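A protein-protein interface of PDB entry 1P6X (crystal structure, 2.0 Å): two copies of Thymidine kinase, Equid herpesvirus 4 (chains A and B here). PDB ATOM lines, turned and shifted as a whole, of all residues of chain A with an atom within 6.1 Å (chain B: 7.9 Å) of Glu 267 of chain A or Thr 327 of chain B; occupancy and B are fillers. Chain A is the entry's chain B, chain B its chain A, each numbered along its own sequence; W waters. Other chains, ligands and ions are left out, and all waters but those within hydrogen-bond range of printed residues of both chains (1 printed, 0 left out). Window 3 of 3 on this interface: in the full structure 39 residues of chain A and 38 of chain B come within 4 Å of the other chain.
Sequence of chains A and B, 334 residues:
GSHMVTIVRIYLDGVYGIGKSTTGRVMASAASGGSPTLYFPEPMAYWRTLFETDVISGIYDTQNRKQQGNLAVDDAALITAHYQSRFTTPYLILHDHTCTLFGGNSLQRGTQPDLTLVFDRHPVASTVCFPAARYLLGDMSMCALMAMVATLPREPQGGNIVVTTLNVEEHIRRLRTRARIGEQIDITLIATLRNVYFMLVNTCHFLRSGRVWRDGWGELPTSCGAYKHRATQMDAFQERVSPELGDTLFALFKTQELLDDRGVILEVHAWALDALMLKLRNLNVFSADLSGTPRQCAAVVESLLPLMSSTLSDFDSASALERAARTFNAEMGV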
ATOM      1  N   ARG A 214      -1.966  29.573  -6.626  1.00  0.00           N
ATOM      2  CA  ARG A 214      -1.936  28.101  -6.616  1.00  0.00           C
ATOM      3  C   ARG A 214      -1.698  27.482  -8.012  1.00  0.00           C
ATOM      4  O   ARG A 214      -1.215  26.357  -8.103  1.00  0.00           O
ATOM      5  CB  ARG A 214      -3.207  27.523  -5.989  1.00  0.00           C
ATOM      6  CG  ARG A 214      -3.329  27.801  -4.486  1.00  0.00           C
ATOM      7  CD  ARG A 214      -4.667  27.417  -3.943  1.00  0.00           C
ATOM      8  NE  ARG A 214      -4.849  27.718  -2.526  1.00  0.00           N
ATOM      9  CZ  ARG A 214      -4.362  26.993  -1.530  1.00  0.00           C
ATOM     10  NH1 ARG A 214      -3.624  25.907  -1.782  1.00  0.00           N
ATOM     11  NH2 ARG A 214      -4.620  27.360  -0.271  1.00  0.00           N
ATOM     12  N   ILE A 265       2.415  24.154   2.231  1.00  0.00           N
ATOM     13  CA  ILE A 265       2.312  25.474   2.859  1.00  0.00           C
ATOM     14  C   ILE A 265       1.247  25.455   3.957  1.00  0.00           C
ATOM     15  O   ILE A 265       0.191  24.866   3.790  1.00  0.00           O
ATOM     16  CB  ILE A 265       2.051  26.619   1.808  1.00  0.00           C
ATOM     17  CG1 ILE A 265       2.280  27.997   2.454  1.00  0.00           C
ATOM     18  CG2 ILE A 265       0.689  26.497   1.154  1.00  0.00           C
ATOM     19  CD1 ILE A 265       2.473  29.156   1.483  1.00  0.00           C
ATOM     20  N   LEU A 266       1.539  26.090   5.082  1.00  0.00           N
ATOM     21  CA  LEU A 266       0.548  26.206   6.154  1.00  0.00           C
ATOM     22  C   LEU A 266      -0.626  27.064   5.670  1.00  0.00           C
ATOM     23  O   LEU A 266      -0.445  28.002   4.890  1.00  0.00           O
ATOM     24  CB  LEU A 266       1.175  26.824   7.405  1.00  0.00           C
ATOM     25  CG  LEU A 266       2.314  26.074   8.116  1.00  0.00           C
ATOM     26  CD1 LEU A 266       2.626  26.750   9.442  1.00  0.00           C
ATOM     27  CD2 LEU A 266       2.007  24.582   8.321  1.00  0.00           C
ATOM     28  N   GLU A 267      -1.828  26.706   6.108  1.00  0.00           N
ATOM     29  CA  GLU A 267      -3.017  27.417   5.716  1.00  0.00           C
ATOM     30  C   GLU A 267      -2.938  28.900   6.053  1.00  0.00           C
ATOM     31  O   GLU A 267      -3.370  29.725   5.260  1.00  0.00           O
ATOM     32  CB  GLU A 267      -4.255  26.751   6.313  1.00  0.00           C
ATOM     33  CG  GLU A 267      -4.776  25.601   5.459  1.00  0.00           C
ATOM     34  CD  GLU A 267      -5.197  26.055   4.062  1.00  0.00           C
ATOM     35  OE1 GLU A 267      -6.201  26.807   3.947  1.00  0.00           O
ATOM     36  OE2 GLU A 267      -4.515  25.666   3.080  1.00  0.00           O
ATOM     37  N   VAL A 268      -2.338  29.246   7.191  1.00  0.00           N
ATOM     38  CA  VAL A 268      -2.225  30.651   7.571  1.00  0.00           C
ATOM     39  C   VAL A 268      -1.338  31.445   6.580  1.00  0.00           C
ATOM     40  O   VAL A 268      -1.602  32.624   6.295  1.00  0.00           O
ATOM     41  CB  VAL A 268      -1.738  30.813   9.043  1.00  0.00           C
ATOM     42  CG1 VAL A 268      -0.332  30.248   9.241  1.00  0.00           C
ATOM     43  CG2 VAL A 268      -1.821  32.276   9.496  1.00  0.00           C
ATOM     44  N   HIS A 269      -0.307  30.786   6.041  1.00  0.00           N
ATOM     45  CA  HIS A 269       0.558  31.448   5.086  1.00  0.00           C
ATOM     46  C   HIS A 269      -0.141  31.516   3.730  1.00  0.00           C
ATOM     47  O   HIS A 269       0.004  32.499   3.014  1.00  0.00           O
ATOM     48  CB  HIS A 269       1.932  30.764   4.987  1.00  0.00           C
ATOM     49  CG  HIS A 269       2.674  30.675   6.291  1.00  0.00           C
ATOM     50  ND1 HIS A 269       2.770  31.728   7.179  1.00  0.00           N
ATOM     51  CD2 HIS A 269       3.378  29.654   6.842  1.00  0.00           C
ATOM     52  CE1 HIS A 269       3.490  31.355   8.224  1.00  0.00           C
ATOM     53  NE2 HIS A 269       3.871  30.101   8.044  1.00  0.00           N
ATOM     54  N   ALA A 270      -0.895  30.473   3.376  1.00  0.00           N
ATOM     55  CA  ALA A 270      -1.745  30.508   2.181  1.00  0.00           C
ATOM     56  C   ALA A 270      -2.717  31.695   2.231  1.00  0.00           C
ATOM     57  O   ALA A 270      -2.928  32.359   1.229  1.00  0.00           O
ATOM     58  CB  ALA A 270      -2.502  29.207   2.009  1.00  0.00           C
ATOM     59  N   TRP A 271      -3.285  31.962   3.410  1.00  0.00           N
ATOM     60  CA  TRP A 271      -4.169  33.126   3.593  1.00  0.00           C
ATOM     61  C   TRP A 271      -3.437  34.421   3.289  1.00  0.00           C
ATOM     62  O   TRP A 271      -4.009  35.328   2.692  1.00  0.00           O
ATOM     63  CB  TRP A 271      -4.770  33.182   5.017  1.00  0.00           C
ATOM     64  CG  TRP A 271      -5.694  32.037   5.367  1.00  0.00           C
ATOM     65  CD1 TRP A 271      -6.197  31.060   4.522  1.00  0.00           C
ATOM     66  CD2 TRP A 271      -6.226  31.747   6.663  1.00  0.00           C
ATOM     67  NE1 TRP A 271      -6.995  30.191   5.231  1.00  0.00           N
ATOM     68  CE2 TRP A 271      -7.024  30.581   6.547  1.00  0.00           C
ATOM     69  CE3 TRP A 271      -6.084  32.345   7.928  1.00  0.00           C
ATOM     70  CZ2 TRP A 271      -7.692  30.011   7.649  1.00  0.00           C
ATOM     71  CZ3 TRP A 271      -6.741  31.782   9.023  1.00  0.00           C
ATOM     72  CH2 TRP A 271      -7.540  30.635   8.872  1.00  0.00           C
ATOM     73  N   ALA A 272      -2.174  34.509   3.684  1.00  0.00           N
ATOM     74  CA  ALA A 272      -1.398  35.727   3.461  1.00  0.00           C
ATOM     75  C   ALA A 272      -1.154  35.975   1.964  1.00  0.00           C
ATOM     76  O   ALA A 272      -1.137  37.122   1.540  1.00  0.00           O
ATOM     77  CB  ALA A 272      -0.086  35.706   4.239  1.00  0.00           C
ATOM     78  N   PHE B  40     -11.688  31.571  17.886  1.00  0.00           N
ATOM     79  CA  PHE B  40     -10.399  31.778  17.227  1.00  0.00           C
ATOM     80  C   PHE B  40      -9.407  32.227  18.299  1.00  0.00           C
ATOM     81  O   PHE B  40      -9.463  33.357  18.774  1.00  0.00           O
ATOM     82  CB  PHE B  40     -10.518  32.873  16.155  1.00  0.00           C
ATOM     83  CG  PHE B  40     -11.393  32.519  14.994  1.00  0.00           C
ATOM     84  CD1 PHE B  40     -12.779  32.697  15.056  1.00  0.00           C
ATOM     85  CD2 PHE B  40     -10.834  32.071  13.815  1.00  0.00           C
ATOM     86  CE1 PHE B  40     -13.586  32.391  13.966  1.00  0.00           C
ATOM     87  CE2 PHE B  40     -11.637  31.769  12.718  1.00  0.00           C
ATOM     88  CZ  PHE B  40     -13.002  31.928  12.796  1.00  0.00           C
ATOM     89  N   PRO B  41      -8.489  31.341  18.675  1.00  0.00           N
ATOM     90  CA  PRO B  41      -7.570  31.594  19.804  1.00  0.00           C
ATOM     91  C   PRO B  41      -6.534  32.671  19.461  1.00  0.00           C
ATOM     92  O   PRO B  41      -6.435  33.029  18.281  1.00  0.00           O
ATOM     93  CB  PRO B  41      -6.851  30.247  19.971  1.00  0.00           C
ATOM     94  CG  PRO B  41      -6.860  29.654  18.582  1.00  0.00           C
ATOM     95  CD  PRO B  41      -8.228  30.054  18.005  1.00  0.00           C
ATOM     96  N   ILE B  93      -3.516  38.900   9.120  1.00  0.00           N
ATOM     97  CA  ILE B  93      -3.792  37.802   8.219  1.00  0.00           C
ATOM     98  C   ILE B  93      -5.185  37.201   8.476  1.00  0.00           C
ATOM     99  O   ILE B  93      -5.954  36.916   7.521  1.00  0.00           O
ATOM    100  CB  ILE B  93      -2.703  36.701   8.340  1.00  0.00           C
ATOM    101  CG1 ILE B  93      -1.360  37.232   7.777  1.00  0.00           C
ATOM    102  CG2 ILE B  93      -3.149  35.438   7.603  1.00  0.00           C
ATOM    103  CD1 ILE B  93      -0.121  36.344   8.129  1.00  0.00           C
ATOM    104  N   HIS B  97      -8.520  37.369   5.951  1.00  0.00           N
ATOM    105  CA  HIS B  97      -9.207  36.143   5.548  1.00  0.00           C
ATOM    106  C   HIS B  97     -10.698  36.163   5.961  1.00  0.00           C
ATOM    107  O   HIS B  97     -11.565  35.846   5.175  1.00  0.00           O
ATOM    108  CB  HIS B  97      -8.501  34.911   6.134  1.00  0.00           C
ATOM    109  CG  HIS B  97      -9.118  33.615   5.717  1.00  0.00           C
ATOM    110  ND1 HIS B  97      -9.085  33.160   4.413  1.00  0.00           N
ATOM    111  CD2 HIS B  97      -9.827  32.698   6.419  1.00  0.00           C
ATOM    112  CE1 HIS B  97      -9.739  32.015   4.332  1.00  0.00           C
ATOM    113  NE2 HIS B  97     -10.195  31.711   5.536  1.00  0.00           N
ATOM    114  N   ALA B 320     -17.028  28.241   5.341  1.00  0.00           N
ATOM    115  CA  ALA B 320     -15.622  28.684   5.226  1.00  0.00           C
ATOM    116  C   ALA B 320     -15.085  29.204   6.565  1.00  0.00           C
ATOM    117  O   ALA B 320     -13.920  28.999   6.888  1.00  0.00           O
ATOM    118  CB  ALA B 320     -15.450  29.752   4.124  1.00  0.00           C
ATOM    119  N   LEU B 321     -15.948  29.853   7.344  1.00  0.00           N
ATOM    120  CA  LEU B 321     -15.575  30.321   8.684  1.00  0.00           C
ATOM    121  C   LEU B 321     -15.307  29.186   9.668  1.00  0.00           C
ATOM    122  O   LEU B 321     -14.342  29.252  10.436  1.00  0.00           O
ATOM    123  CB  LEU B 321     -16.620  31.311   9.242  1.00  0.00           C
ATOM    124  CG  LEU B 321     -16.567  32.717   8.652  1.00  0.00           C
ATOM    125  CD1 LEU B 321     -17.915  33.444   8.854  1.00  0.00           C
ATOM    126  CD2 LEU B 321     -15.439  33.549   9.273  1.00  0.00           C
ATOM    127  N   GLU B 322     -16.145  28.144   9.622  1.00  0.00           N
ATOM    128  CA  GLU B 322     -15.964  26.915  10.415  1.00  0.00           C
ATOM    129  C   GLU B 322     -14.611  26.256  10.057  1.00  0.00           C
ATOM    130  O   GLU B 322     -13.827  25.896  10.947  1.00  0.00           O
ATOM    131  CB  GLU B 322     -17.189  25.963  10.225  1.00  0.00           C
ATOM    132  CG  GLU B 322     -17.023  24.491  10.659  1.00  0.00           C
ATOM    133  CD  GLU B 322     -17.639  24.134  12.015  1.00  0.00           C
ATOM    134  OE1 GLU B 322     -18.679  24.683  12.398  1.00  0.00           O
ATOM    135  OE2 GLU B 322     -17.078  23.269  12.738  1.00  0.00           O
ATOM    136  N   ARG B 323     -14.330  26.144   8.759  1.00  0.00           N
ATOM    137  CA  ARG B 323     -13.042  25.613   8.293  1.00  0.00           C
ATOM    138  C   ARG B 323     -11.891  26.487   8.777  1.00  0.00           C
ATOM    139  O   ARG B 323     -10.837  25.970   9.170  1.00  0.00           O
ATOM    140  CB  ARG B 323     -13.004  25.487   6.754  1.00  0.00           C
ATOM    141  CG  ARG B 323     -13.823  24.330   6.194  1.00  0.00           C
ATOM    142  CD  ARG B 323     -13.598  24.025   4.685  1.00  0.00           C
ATOM    143  NE  ARG B 323     -13.599  25.225   3.838  1.00  0.00           N
ATOM    144  CZ  ARG B 323     -14.680  25.741   3.250  1.00  0.00           C
ATOM    145  NH1 ARG B 323     -15.868  25.175   3.395  1.00  0.00           N
ATOM    146  NH2 ARG B 323     -14.563  26.820   2.489  1.00  0.00           N
ATOM    147  N   ALA B 324     -12.093  27.815   8.742  1.00  0.00           N
ATOM    148  CA  ALA B 324     -11.102  28.778   9.209  1.00  0.00           C
ATOM    149  C   ALA B 324     -10.795  28.593  10.687  1.00  0.00           C
ATOM    150  O   ALA B 324      -9.622  28.585  11.085  1.00  0.00           O
ATOM    151  CB  ALA B 324     -11.552  30.234   8.927  1.00  0.00           C
ATOM    152  N   ALA B 325     -11.837  28.471  11.506  1.00  0.00           N
ATOM    153  CA  ALA B 325     -11.655  28.248  12.935  1.00  0.00           C
ATOM    154  C   ALA B 325     -10.903  26.949  13.206  1.00  0.00           C
ATOM    155  O   ALA B 325     -10.021  26.923  14.050  1.00  0.00           O
ATOM    156  CB  ALA B 325     -12.983  28.255  13.670  1.00  0.00           C
ATOM    157  N   ARG B 326     -11.279  25.873  12.522  1.00  0.00           N
ATOM    158  CA  ARG B 326     -10.621  24.578  12.743  1.00  0.00           C
ATOM    159  C   ARG B 326      -9.154  24.654  12.399  1.00  0.00           C
ATOM    160  O   ARG B 326      -8.309  24.163  13.139  1.00  0.00           O
ATOM    161  CB  ARG B 326     -11.293  23.472  11.934  1.00  0.00           C
ATOM    162  CG  ARG B 326     -12.604  23.052  12.524  1.00  0.00           C
ATOM    163  CD  ARG B 326     -12.925  21.582  12.354  1.00  0.00           C
ATOM    164  NE  ARG B 326     -14.349  21.375  12.108  1.00  0.00           N
ATOM    165  CZ  ARG B 326     -14.899  21.318  10.899  1.00  0.00           C
ATOM    166  NH1 ARG B 326     -14.146  21.461   9.800  1.00  0.00           N
ATOM    167  NH2 ARG B 326     -16.210  21.118  10.791  1.00  0.00           N
ATOM    168  N   THR B 327      -8.865  25.291  11.267  1.00  0.00           N
ATOM    169  CA  THR B 327      -7.494  25.504  10.770  1.00  0.00           C
ATOM    170  C   THR B 327      -6.653  26.382  11.685  1.00  0.00           C
ATOM    171  O   THR B 327      -5.471  26.075  11.963  1.00  0.00           O
ATOM    172  CB  THR B 327      -7.557  26.145   9.349  1.00  0.00           C
ATOM    173  OG1 THR B 327      -7.927  25.137   8.394  1.00  0.00           O
ATOM    174  CG2 THR B 327      -6.204  26.584   8.926  1.00  0.00           C
ATOM    175  N   PHE B 328      -7.236  27.502  12.128  1.00  0.00           N
ATOM    176  CA  PHE B 328      -6.532  28.407  13.021  1.00  0.00           C
ATOM    177  C   PHE B 328      -6.313  27.764  14.393  1.00  0.00           C
ATOM    178  O   PHE B 328      -5.250  27.905  14.957  1.00  0.00           O
ATOM    179  CB  PHE B 328      -7.285  29.728  13.178  1.00  0.00           C
ATOM    180  CG  PHE B 328      -6.412  30.917  13.506  1.00  0.00           C
ATOM    181  CD1 PHE B 328      -6.532  31.554  14.738  1.00  0.00           C
ATOM    182  CD2 PHE B 328      -5.534  31.449  12.562  1.00  0.00           C
ATOM    183  CE1 PHE B 328      -5.794  32.680  15.029  1.00  0.00           C
ATOM    184  CE2 PHE B 328      -4.786  32.578  12.848  1.00  0.00           C
ATOM    185  CZ  PHE B 328      -4.910  33.195  14.081  1.00  0.00           C
ATOM    186  N   ASN B 329      -7.305  27.049  14.921  1.00  0.00           N
ATOM    187  CA  ASN B 329      -7.108  26.346  16.186  1.00  0.00           C
ATOM    188  C   ASN B 329      -5.965  25.315  16.078  1.00  0.00           C
ATOM    189  O   ASN B 329      -5.081  25.271  16.938  1.00  0.00           O
ATOM    190  CB  ASN B 329      -8.391  25.680  16.668  1.00  0.00           C
ATOM    191  CG  ASN B 329      -9.268  26.625  17.479  1.00  0.00           C
ATOM    192  OD1 ASN B 329      -9.122  26.752  18.694  1.00  0.00           O
ATOM    193  ND2 ASN B 329     -10.166  27.306  16.797  1.00  0.00           N
ATOM    194  N   ALA B 330      -5.967  24.545  14.990  1.00  0.00           N
ATOM    195  CA  ALA B 330      -4.958  23.494  14.778  1.00  0.00           C
ATOM    196  C   ALA B 330      -3.567  24.064  14.555  1.00  0.00           C
ATOM    197  O   ALA B 330      -2.617  23.668  15.233  1.00  0.00           O
ATOM    198  CB  ALA B 330      -5.360  22.581  13.622  1.00  0.00           C
ATOM    199  N   GLU B 331      -3.438  25.000  13.620  1.00  0.00           N
ATOM    200  CA  GLU B 331      -2.125  25.571  13.300  1.00  0.00           C
ATOM    201  C   GLU B 331      -1.540  26.469  14.392  1.00  0.00           C
ATOM    202  O   GLU B 331      -0.321  26.559  14.511  1.00  0.00           O
ATOM    203  CB  GLU B 331      -2.130  26.290  11.945  1.00  0.00           C
ATOM    204  CG  GLU B 331      -2.586  25.424  10.773  1.00  0.00           C
ATOM    205  CD  GLU B 331      -2.296  26.043   9.402  1.00  0.00           C
ATOM    206  OE1 GLU B 331      -2.082  27.282   9.317  1.00  0.00           O
ATOM    207  OE2 GLU B 331      -2.284  25.278   8.404  1.00  0.00           O
ATOM    208  N   MET B 332      -2.390  27.149  15.171  1.00  0.00           N
ATOM    209  CA  MET B 332      -1.908  28.075  16.218  1.00  0.00           C
ATOM    210  C   MET B 332      -1.612  27.415  17.579  1.00  0.00           C
ATOM    211  O   MET B 332      -1.021  28.033  18.476  1.00  0.00           O
ATOM    212  CB  MET B 332      -2.865  29.271  16.407  1.00  0.00           C
ATOM    213  CG  MET B 332      -3.005  30.181  15.162  1.00  0.00           C
ATOM    214  SD  MET B 332      -1.431  30.932  14.637  1.00  0.00           S
ATOM    215  CE  MET B 332      -1.025  29.957  13.210  1.00  0.00           C
ATOM    216  N   GLY B 333      -2.007  26.155  17.706  1.00  0.00           N
ATOM    217  CA  GLY B 333      -1.778  25.385  18.920  1.00  0.00           C
ATOM    218  C   GLY B 333      -0.333  25.288  19.389  1.00  0.00           C
ATOM    219  O   GLY B 333       0.604  25.246  18.573  1.00  0.00           O
HETATM  220  O   HOH W   1      -4.967  36.905   4.883  1.00  0.00           O
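The side-chain carboxylate (OE2) of Glu 331 of chain B lies within hydrogen-bond range of the backbone NH (N) of Glu 267 of chain A.
OE1 of Glu 331 of chain B lies within hydrogen-bond range of N of Val 268 of chain A.
OG1 of Thr 327 of chain B is in hydrogen-bond range of O of Arg 323 of chain B (3.1 Å).
The guanidinium group (NH2) of Arg 214 of chain A is in salt-bridge range of the side-chain carboxylate (OE2) of Glu 267 of chain A (3.8 Å).
Leu 266 of chain A touches Glu 331 of chain B.
Thr 327 of chain B touches Glu 267 of chain A.
Ile 93 of chain B touches Val 268 of chain A.
Ile 93 of chain B touches Trp 271 of chain A.
Trp 271 of chain A touches His 97 of chain B (NE1 to CE1, 3.4 Å).
Trp 271 of chain A touches Ala 324 of chain B.
CZ2 of Trp 271 of chain A touches CG2 of Thr 327 of chain B (3.9 Å).
Trp 271 of chain A touches Phe 328 of chain B (CZ3 to CD2, 3.8 Å).
Ala 272 of chain A touches Ile 93 of chain B (CB to CD1, 3.9 Å).
Glu 267 of chain A touches just these residues of chain B: Thr 327 (3.3 Å) and Glu 331 (2.7 Å).
Of the printed residues of chain A, Phe 328 of chain B touches Trp 271 (3.8 Å).
Of the printed residues of chain B, Leu 266 of chain A touches Glu 331 (3.7 Å).
Of the printed residues of chain A, Ala 324 of chain B touches Trp 271 (3.7 Å).
Asn 329 of chain B touches none of the printed residues of chain A.
Ile 265 of chain A touches none of the printed residues of chain B.
The nearest residue of chain B that does not touch Glu 267 of chain A is Ile 93 of chain B (6.2 Å).
Hydrophobic or aromatic side chains of chain B that line the printed part of chain A: Ile 93, His 97 and Phe 328.
Of the 9 printed residues of chain A, 5 touch a printed residue of chain B.
Along chain A the printed residues that touch a printed residue of chain B span positions 266 to 272.
Among the printed residues, 11 pairs touch across the chains.
Among the printed residues, no Asp or Glu carboxylate lies within 4 Å of a Lys or Arg side-chain nitrogen of the other chain.
No position is printed for both chains.
Water W1 bridges O of Ile 93 of chain B (2.8 Å) and O of Trp 271 of chain A (2.9 Å).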
